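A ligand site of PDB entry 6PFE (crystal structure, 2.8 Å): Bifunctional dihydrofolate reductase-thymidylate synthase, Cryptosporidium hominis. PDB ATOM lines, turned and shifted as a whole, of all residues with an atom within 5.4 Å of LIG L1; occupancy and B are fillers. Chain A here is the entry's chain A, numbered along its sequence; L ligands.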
ATOM      1  N   ARG A 257     -14.406  18.530  15.320  1.00  0.00           N
ATOM      2  CA  ARG A 257     -15.088  17.247  15.484  1.00  0.00           C
ATOM      3  C   ARG A 257     -14.578  16.479  16.704  1.00  0.00           C
ATOM      4  O   ARG A 257     -15.308  15.656  17.263  1.00  0.00           O
ATOM      5  CB  ARG A 257     -14.916  16.399  14.231  1.00  0.00           C
ATOM      6  CG  ARG A 257     -13.465  16.043  13.984  1.00  0.00           C
ATOM      7  CD  ARG A 257     -13.266  15.111  12.809  1.00  0.00           C
ATOM      8  NE  ARG A 257     -11.838  14.907  12.587  1.00  0.00           N
ATOM      9  CZ  ARG A 257     -11.098  14.063  13.302  1.00  0.00           C
ATOM     10  NH1 ARG A 257     -11.652  13.358  14.274  1.00  0.00           N
ATOM     11  NH2 ARG A 257      -9.801  13.935  13.038  1.00  0.00           N
ATOM     12  N   LYS A 284      12.988  18.704  16.283  1.00  0.00           N
ATOM     13  CA  LYS A 284      12.431  17.599  17.038  1.00  0.00           C
ATOM     14  C   LYS A 284      12.757  16.320  16.279  1.00  0.00           C
ATOM     15  O   LYS A 284      12.726  16.293  15.044  1.00  0.00           O
ATOM     16  CB  LYS A 284      10.926  17.733  17.261  1.00  0.00           C
ATOM     17  CG  LYS A 284      10.062  17.305  16.086  1.00  0.00           C
ATOM     18  CD  LYS A 284       8.588  17.387  16.432  1.00  0.00           C
ATOM     19  CE  LYS A 284       7.735  17.247  15.195  1.00  0.00           C
ATOM     20  NZ  LYS A 284       6.323  17.640  15.463  1.00  0.00           N
ATOM     21  N   LYS A 285      13.097  15.265  17.012  1.00  0.00           N
ATOM     22  CA  LYS A 285      13.403  13.976  16.382  1.00  0.00           C
ATOM     23  C   LYS A 285      12.118  13.419  15.778  1.00  0.00           C
ATOM     24  O   LYS A 285      11.251  12.906  16.480  1.00  0.00           O
ATOM     25  CB  LYS A 285      13.998  13.022  17.407  1.00  0.00           C
ATOM     26  CG  LYS A 285      14.555  11.734  16.814  1.00  0.00           C
ATOM     27  CD  LYS A 285      15.221  10.886  17.890  1.00  0.00           C
ATOM     28  CE  LYS A 285      15.697   9.558  17.323  1.00  0.00           C
ATOM     29  NZ  LYS A 285      16.478   8.771  18.315  1.00  0.00           N
ATOM     30  N   ALA A 287       9.926  10.828  13.717  1.00  0.00           N
ATOM     31  CA  ALA A 287       9.936   9.388  13.448  1.00  0.00           C
ATOM     32  C   ALA A 287       9.882   9.168  11.940  1.00  0.00           C
ATOM     33  O   ALA A 287       8.824   8.947  11.346  1.00  0.00           O
ATOM     34  CB  ALA A 287       8.763   8.711  14.157  1.00  0.00           C
ATOM     35  N   SER A 290       8.342   5.696  10.548  1.00  0.00           N
ATOM     36  CA  SER A 290       6.887   5.594  10.483  1.00  0.00           C
ATOM     37  C   SER A 290       6.328   6.370   9.295  1.00  0.00           C
ATOM     38  O   SER A 290       5.332   5.947   8.684  1.00  0.00           O
ATOM     39  CB  SER A 290       6.255   6.093  11.777  1.00  0.00           C
ATOM     40  OG  SER A 290       6.834   5.453  12.908  1.00  0.00           O
ATOM     41  N   GLU A 294       4.086   4.409   6.318  1.00  0.00           N
ATOM     42  CA  GLU A 294       2.753   4.869   5.944  1.00  0.00           C
ATOM     43  C   GLU A 294       2.688   5.206   4.457  1.00  0.00           C
ATOM     44  O   GLU A 294       1.660   4.983   3.804  1.00  0.00           O
ATOM     45  CB  GLU A 294       2.382   6.099   6.767  1.00  0.00           C
ATOM     46  CG  GLU A 294       1.006   6.669   6.425  1.00  0.00           C
ATOM     47  CD  GLU A 294       0.875   8.116   6.845  1.00  0.00           C
ATOM     48  OE1 GLU A 294       1.876   8.854   6.736  1.00  0.00           O
ATOM     49  OE2 GLU A 294      -0.235   8.512   7.275  1.00  0.00           O
ATOM     50  N   TYR A 314       1.800   3.005  14.733  1.00  0.00           N
ATOM     51  CA  TYR A 314       0.506   3.150  15.389  1.00  0.00           C
ATOM     52  C   TYR A 314      -0.138   4.504  15.125  1.00  0.00           C
ATOM     53  O   TYR A 314      -0.956   4.965  15.927  1.00  0.00           O
ATOM     54  CB  TYR A 314       0.651   2.926  16.898  1.00  0.00           C
ATOM     55  CG  TYR A 314       1.522   1.752  17.291  1.00  0.00           C
ATOM     56  CD1 TYR A 314       1.025   0.453  17.255  1.00  0.00           C
ATOM     57  CD2 TYR A 314       2.836   1.942  17.707  1.00  0.00           C
ATOM     58  CE1 TYR A 314       1.813  -0.612  17.619  1.00  0.00           C
ATOM     59  CE2 TYR A 314       3.630   0.880  18.077  1.00  0.00           C
ATOM     60  CZ  TYR A 314       3.111  -0.406  18.029  1.00  0.00           C
ATOM     61  OH  TYR A 314       3.897  -1.484  18.399  1.00  0.00           O
ATOM     62  N   ILE A 315       0.179   5.147  14.004  1.00  0.00           N
ATOM     63  CA  ILE A 315      -0.361   6.481  13.759  1.00  0.00           C
ATOM     64  C   ILE A 315      -1.827   6.419  13.349  1.00  0.00           C
ATOM     65  O   ILE A 315      -2.536   7.430  13.460  1.00  0.00           O
ATOM     66  CB  ILE A 315       0.447   7.236  12.685  1.00  0.00           C
ATOM     67  CG1 ILE A 315       0.253   6.606  11.311  1.00  0.00           C
ATOM     68  CG2 ILE A 315       1.910   7.268  13.051  1.00  0.00           C
ATOM     69  CD1 ILE A 315       0.942   7.376  10.205  1.00  0.00           C
ATOM     70  N   TRP A 316      -2.312   5.267  12.888  1.00  0.00           N
ATOM     71  CA  TRP A 316      -3.710   5.112  12.503  1.00  0.00           C
ATOM     72  C   TRP A 316      -4.479   4.250  13.503  1.00  0.00           C
ATOM     73  O   TRP A 316      -5.509   3.676  13.148  1.00  0.00           O
ATOM     74  CB  TRP A 316      -3.816   4.526  11.096  1.00  0.00           C
ATOM     75  CG  TRP A 316      -3.510   5.516  10.004  1.00  0.00           C
ATOM     76  CD1 TRP A 316      -2.325   5.673   9.362  1.00  0.00           C
ATOM     77  CD2 TRP A 316      -4.422   6.457   9.415  1.00  0.00           C
ATOM     78  NE1 TRP A 316      -2.429   6.669   8.409  1.00  0.00           N
ATOM     79  CE2 TRP A 316      -3.705   7.162   8.424  1.00  0.00           C
ATOM     80  CE3 TRP A 316      -5.764   6.777   9.638  1.00  0.00           C
ATOM     81  CZ2 TRP A 316      -4.290   8.171   7.665  1.00  0.00           C
ATOM     82  CZ3 TRP A 316      -6.332   7.784   8.877  1.00  0.00           C
ATOM     83  CH2 TRP A 316      -5.602   8.461   7.897  1.00  0.00           C
ATOM     84  N   ASN A 319      -7.803   6.647  14.909  1.00  0.00           N
ATOM     85  CA  ASN A 319      -8.882   6.665  13.920  1.00  0.00           C
ATOM     86  C   ASN A 319      -9.242   5.276  13.421  1.00  0.00           C
ATOM     87  O   ASN A 319      -9.960   5.141  12.430  1.00  0.00           O
ATOM     88  CB  ASN A 319      -8.478   7.554  12.737  1.00  0.00           C
ATOM     89  CG  ASN A 319      -8.042   8.940  13.174  1.00  0.00           C
ATOM     90  OD1 ASN A 319      -6.873   9.162  13.488  1.00  0.00           O
ATOM     91  ND2 ASN A 319      -8.990   9.870  13.205  1.00  0.00           N
ATOM     92  N   LEU A 399     -11.763   8.533   7.792  1.00  0.00           N
ATOM     93  CA  LEU A 399     -11.384   9.924   7.914  1.00  0.00           C
ATOM     94  C   LEU A 399     -11.223  10.490   6.508  1.00  0.00           C
ATOM     95  O   LEU A 399     -10.554   9.875   5.666  1.00  0.00           O
ATOM     96  CB  LEU A 399     -10.095  10.075   8.727  1.00  0.00           C
ATOM     97  CG  LEU A 399      -9.742  11.489   9.164  1.00  0.00           C
ATOM     98  CD1 LEU A 399     -10.814  12.007  10.103  1.00  0.00           C
ATOM     99  CD2 LEU A 399      -8.382  11.521   9.829  1.00  0.00           C
ATOM    100  N   ASP A 426      -2.670  19.479  10.954  1.00  0.00           N
ATOM    101  CA  ASP A 426      -2.324  19.368  12.363  1.00  0.00           C
ATOM    102  C   ASP A 426      -0.840  19.685  12.524  1.00  0.00           C
ATOM    103  O   ASP A 426       0.013  18.803  12.453  1.00  0.00           O
ATOM    104  CB  ASP A 426      -2.659  17.979  12.891  1.00  0.00           C
ATOM    105  CG  ASP A 426      -2.224  17.763  14.322  1.00  0.00           C
ATOM    106  OD1 ASP A 426      -1.818  18.737  14.991  1.00  0.00           O
ATOM    107  OD2 ASP A 426      -2.297  16.611  14.789  1.00  0.00           O
ATOM    108  N   GLY A 428       2.362  20.042  14.375  1.00  0.00           N
ATOM    109  CA  GLY A 428       2.777  19.342  15.579  1.00  0.00           C
ATOM    110  C   GLY A 428       2.809  17.849  15.398  1.00  0.00           C
ATOM    111  O   GLY A 428       3.737  17.181  15.868  1.00  0.00           O
ATOM    112  N   LEU A 429       1.795  17.291  14.723  1.00  0.00           N
ATOM    113  CA  LEU A 429       1.786  15.857  14.414  1.00  0.00           C
ATOM    114  C   LEU A 429       1.716  15.619  12.912  1.00  0.00           C
ATOM    115  O   LEU A 429       2.686  15.105  12.344  1.00  0.00           O
ATOM    116  CB  LEU A 429       0.618  15.170  15.136  1.00  0.00           C
ATOM    117  CG  LEU A 429       0.730  15.084  16.657  1.00  0.00           C
ATOM    118  CD1 LEU A 429      -0.377  14.219  17.221  1.00  0.00           C
ATOM    119  CD2 LEU A 429       2.084  14.552  17.067  1.00  0.00           C
ATOM    120  N   GLY A 430       0.616  15.983  12.245  1.00  0.00           N
ATOM    121  CA  GLY A 430       0.477  15.636  10.841  1.00  0.00           C
ATOM    122  C   GLY A 430       1.423  16.394   9.935  1.00  0.00           C
ATOM    123  O   GLY A 430       1.975  15.835   8.984  1.00  0.00           O
ATOM    124  N   PHE A 433       4.886  15.141   9.364  1.00  0.00           N
ATOM    125  CA  PHE A 433       4.737  13.923   8.567  1.00  0.00           C
ATOM    126  C   PHE A 433       4.435  14.257   7.119  1.00  0.00           C
ATOM    127  O   PHE A 433       5.049  13.701   6.206  1.00  0.00           O
ATOM    128  CB  PHE A 433       3.637  13.046   9.172  1.00  0.00           C
ATOM    129  CG  PHE A 433       4.112  12.140  10.273  1.00  0.00           C
ATOM    130  CD1 PHE A 433       4.855  12.646  11.320  1.00  0.00           C
ATOM    131  CD2 PHE A 433       3.819  10.790  10.254  1.00  0.00           C
ATOM    132  CE1 PHE A 433       5.296  11.821  12.337  1.00  0.00           C
ATOM    133  CE2 PHE A 433       4.264   9.956  11.269  1.00  0.00           C
ATOM    134  CZ  PHE A 433       4.996  10.469  12.311  1.00  0.00           C
ATOM    135  N   TYR A 466      -3.577  22.156  17.962  1.00  0.00           N
ATOM    136  CA  TYR A 466      -4.438  21.666  19.021  1.00  0.00           C
ATOM    137  C   TYR A 466      -3.984  22.220  20.363  1.00  0.00           C
ATOM    138  O   TYR A 466      -2.786  22.372  20.615  1.00  0.00           O
ATOM    139  CB  TYR A 466      -4.452  20.142  19.047  1.00  0.00           C
ATOM    140  CG  TYR A 466      -5.288  19.544  17.937  1.00  0.00           C
ATOM    141  CD1 TYR A 466      -4.744  19.287  16.686  1.00  0.00           C
ATOM    142  CD2 TYR A 466      -6.627  19.237  18.142  1.00  0.00           C
ATOM    143  CE1 TYR A 466      -5.515  18.743  15.667  1.00  0.00           C
ATOM    144  CE2 TYR A 466      -7.401  18.701  17.137  1.00  0.00           C
ATOM    145  CZ  TYR A 466      -6.853  18.455  15.908  1.00  0.00           C
ATOM    146  OH  TYR A 466      -7.656  17.916  14.919  1.00  0.00           O
ATOM    147  N   THR A 514      13.060  14.258  20.803  1.00  0.00           N
ATOM    148  CA  THR A 514      11.674  14.123  20.382  1.00  0.00           C
ATOM    149  C   THR A 514      10.751  14.828  21.364  1.00  0.00           C
ATOM    150  O   THR A 514      11.075  15.007  22.537  1.00  0.00           O
ATOM    151  CB  THR A 514      11.296  12.645  20.262  1.00  0.00           C
ATOM    152  OG1 THR A 514       9.932  12.530  19.855  1.00  0.00           O
ATOM    153  CG2 THR A 514      11.486  11.938  21.596  1.00  0.00           C
ATOM    154  N   ILE A 515       9.579  15.231  20.875  1.00  0.00           N
ATOM    155  CA  ILE A 515       8.582  15.943  21.664  1.00  0.00           C
ATOM    156  C   ILE A 515       7.280  15.160  21.594  1.00  0.00           C
ATOM    157  O   ILE A 515       6.700  15.021  20.508  1.00  0.00           O
ATOM    158  CB  ILE A 515       8.379  17.380  21.165  1.00  0.00           C
ATOM    159  CG1 ILE A 515       9.711  18.140  21.153  1.00  0.00           C
ATOM    160  CG2 ILE A 515       7.380  18.104  22.041  1.00  0.00           C
ATOM    161  CD1 ILE A 515       9.598  19.527  20.566  1.00  0.00           C
ATOM    162  N   LYS A 516       6.823  14.649  22.735  1.00  0.00           N
ATOM    163  CA  LYS A 516       5.619  13.835  22.769  1.00  0.00           C
ATOM    164  C   LYS A 516       4.387  14.724  22.677  1.00  0.00           C
ATOM    165  O   LYS A 516       4.252  15.694  23.431  1.00  0.00           O
ATOM    166  CB  LYS A 516       5.583  12.987  24.033  1.00  0.00           C
ATOM    167  N   MET A 517       3.480  14.383  21.767  1.00  0.00           N
ATOM    168  CA  MET A 517       2.241  15.125  21.560  1.00  0.00           C
ATOM    169  C   MET A 517       1.115  14.146  21.280  1.00  0.00           C
ATOM    170  O   MET A 517       1.233  13.316  20.373  1.00  0.00           O
ATOM    171  CB  MET A 517       2.388  16.114  20.395  1.00  0.00           C
ATOM    172  CG  MET A 517       3.123  17.404  20.739  1.00  0.00           C
ATOM    173  SD  MET A 517       3.406  18.440  19.283  1.00  0.00           S
ATOM    174  CE  MET A 517       4.966  17.781  18.696  1.00  0.00           C
ATOM    175  N   MET A 519      -2.410  12.665  19.994  1.00  0.00           N
ATOM    176  CA  MET A 519      -3.237  12.862  18.826  1.00  0.00           C
ATOM    177  C   MET A 519      -4.698  12.988  19.231  1.00  0.00           C
ATOM    178  O   MET A 519      -5.189  12.236  20.081  1.00  0.00           O
ATOM    179  CB  MET A 519      -3.079  11.718  17.819  1.00  0.00           C
ATOM    180  CG  MET A 519      -3.878  11.927  16.543  1.00  0.00           C
ATOM    181  SD  MET A 519      -4.185  10.416  15.620  1.00  0.00           S
ATOM    182  CE  MET A 519      -5.263   9.562  16.772  1.00  0.00           C
ATOM    183  N   ALA A 520      -5.402  13.930  18.605  1.00  0.00           N
ATOM    184  CA  ALA A 520      -6.824  14.123  18.840  1.00  0.00           C
ATOM    185  C   ALA A 520      -7.606  13.164  17.944  1.00  0.00           C
ATOM    186  O   ALA A 520      -7.532  13.263  16.716  1.00  0.00           O
ATOM    187  CB  ALA A 520      -7.222  15.568  18.584  1.00  0.00           C
HETATM  188  C1  LIG L   1       0.463  11.320  12.044  1.00  0.00           C
HETATM  189  C2  LIG L   1       1.273  11.220  13.162  1.00  0.00           C
HETATM  190  C3  LIG L   1       0.794  10.662  14.344  1.00  0.00           C
HETATM  191  C4  LIG L   1      -0.532  10.210  14.396  1.00  0.00           C
HETATM  192  C5  LIG L   1       1.693  10.583  15.556  1.00  0.00           C
HETATM  193  C6  LIG L   1       4.193  10.896  16.023  1.00  0.00           C
HETATM  194  C7  LIG L   1       4.746   8.401  15.981  1.00  0.00           C
HETATM  195  C8  LIG L   1      -3.621  12.254  12.039  1.00  0.00           C
HETATM  196  C9  LIG L   1      -3.000  13.446  12.627  1.00  0.00           C
HETATM  197  C10 LIG L   1      -3.136  11.171  11.281  1.00  0.00           C
HETATM  198  C11 LIG L   1      -4.211  10.335  11.013  1.00  0.00           C
HETATM  199  C12 LIG L   1      -4.980  12.039  12.230  1.00  0.00           C
HETATM  200  C13 LIG L   1      -5.288  13.912  13.443  1.00  0.00           C
HETATM  201  C14 LIG L   1       4.554  12.173  16.430  1.00  0.00           C
HETATM  202  C15 LIG L   1       5.701  12.385  17.187  1.00  0.00           C
HETATM  203  C16 LIG L   1       6.518  11.324  17.534  1.00  0.00           C
HETATM  204  C17 LIG L   1       6.174  10.044  17.125  1.00  0.00           C
HETATM  205  C18 LIG L   1       5.024   9.820  16.361  1.00  0.00           C
HETATM  206  C19 LIG L   1       5.955  14.588  16.552  1.00  0.00           C
HETATM  207  C20 LIG L   1      -1.707  10.977  10.846  1.00  0.00           C
HETATM  208  C21 LIG L   1      -0.850  10.855  12.073  1.00  0.00           C
HETATM  209  C22 LIG L   1      -1.339  10.302  13.263  1.00  0.00           C
HETATM  210  N1  LIG L   1      -3.945  14.183  13.293  1.00  0.00           N
HETATM  211  N2  LIG L   1      -5.820  12.856  12.921  1.00  0.00           N
HETATM  212  N3  LIG L   1      -5.340  10.873  11.602  1.00  0.00           N
HETATM  213  N4  LIG L   1      -6.077  14.878  14.204  1.00  0.00           N
HETATM  214  N5  LIG L   1       2.965  10.817  15.210  1.00  0.00           N
HETATM  215  O1  LIG L   1      -1.837  13.810  12.582  1.00  0.00           O
HETATM  216  O2  LIG L   1       1.318  10.331  16.692  1.00  0.00           O
HETATM  217  O3  LIG L   1       5.750   7.603  16.451  1.00  0.00           O
HETATM  218  O4  LIG L   1       3.781   7.961  15.360  1.00  0.00           O
HETATM  219  O5  LIG L   1       6.020  13.667  17.576  1.00  0.00           O
HETATM  220  N1  LG2 L   2      -4.113  15.549   9.725  1.00  0.00           N
HETATM  221  C1  LG2 L   2      -3.202  16.107   8.887  1.00  0.00           C
HETATM  222  N2  LG2 L   2      -2.573  15.350   7.960  1.00  0.00           N
HETATM  223  C2  LG2 L   2      -2.815  14.033   7.846  1.00  0.00           C
HETATM  224  C3  LG2 L   2      -3.759  13.434   8.720  1.00  0.00           C
HETATM  225  C4  LG2 L   2      -4.370  14.200   9.639  1.00  0.00           C
HETATM  226  O1  LG2 L   2      -2.893  17.288   8.908  1.00  0.00           O
HETATM  227  O2  LG2 L   2      -2.230  13.379   7.000  1.00  0.00           O
HETATM  228  F1  LG2 L   2      -4.067  12.113   8.661  1.00  0.00           F
HETATM  229  C5  LG2 L   2      -4.882  16.205  10.805  1.00  0.00           C
HETATM  230  C6  LG2 L   2      -5.457  17.606  10.496  1.00  0.00           C
HETATM  231  C7  LG2 L   2      -6.652  17.656  11.472  1.00  0.00           C
HETATM  232  C8  LG2 L   2      -7.198  16.220  11.361  1.00  0.00           C
HETATM  233  O3  LG2 L   2      -6.217  17.880  12.810  1.00  0.00           O
HETATM  234  O4  LG2 L   2      -6.049  15.385  11.071  1.00  0.00           O
HETATM  235  C9  LG2 L   2      -8.224  16.144  10.234  1.00  0.00           C
HETATM  236  O5  LG2 L   2      -9.497  15.813  10.766  1.00  0.00           O
HETATM  237  P1  LG2 L   2     -10.532  16.924  10.239  1.00  0.00           P
HETATM  238  O6  LG2 L   2     -10.995  17.826  11.490  1.00  0.00           O
HETATM  239  O7  LG2 L   2      -9.899  17.791   9.229  1.00  0.00           O
HETATM  240  O8  LG2 L   2     -11.795  16.197   9.559  1.00  0.00           O
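The side-chain amide oxygen (OD1) of Asn 319 lies within hydrogen-bond range of a nitrogen (N3) of LIG L1 (3.0 Å). N1 of LIG L1 sits at hydrogen-bond distance from OD2 of Asp 426 (3.3 Å). N of Gly 430 sits at hydrogen-bond distance from O1 of LIG L1, 3.3 Å away. A nitrogen (N4) of LIG L1 is in hydrogen-bond range of the backbone carbonyl oxygen (O) of Ala 520. The side-chain hydroxyl (OH) of Tyr 466 lies within hydrogen-bond range of a nitrogen (N4) of LIG L1 (3.5 Å). The backbone NH of Asp 426 is in hydrogen-bond range of an oxygen (O1) of LG2 L2 (3.0 Å). O3 of LG2 L2 lies within hydrogen-bond range of OH of Tyr 466 (2.6 Å). NE of Arg 257 is in salt-bridge range of O6 of LG2 L2.
N4 of LIG L1 lies close to O4 of LG2 L2, 3.2 Å away.
The side-chain sulfur of Met 519 sits close to the side-chain amide oxygen of Asn 319 (3.7 Å). O of Gly 428 sits at hydrogen-bond distance from NZ of Lys 284, 2.7 Å away. The side-chain carboxylate of Glu 294 sits at hydrogen-bond distance from the indole nitrogen of Trp 316, 3.1 Å away.
O of Ile 515 lies close to O5 of LIG L1, at 3.3 Å. Merely in contact with LIG L1: Lys 284 (3.3 Å), Ala 287 (3.9 Å), Ile 315 (3.1 Å), Trp 316 (3.9 Å), Leu 399 (3.6 Å), Gly 428 (3.5 Å), Leu 429 (3.5 Å), Phe 433 (3.6 Å), Met 517 (3.97 Å) and Met 519 (3.7 Å). Hydrophobic or aromatic side chains that line LIG L1: Ala 287, Ile 315, Trp 316, Leu 399, Leu 429, Phe 433, Met 517 and Met 519. Within 4 Å of LIG L1: Lys 284, Ala 287, Ile 315, Trp 316, Asn 319, Leu 399, Asp 426, Gly 428, Leu 429, Gly 430, Phe 433, Tyr 466, Ile 515, Met 517, Met 519 and Ala 520.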
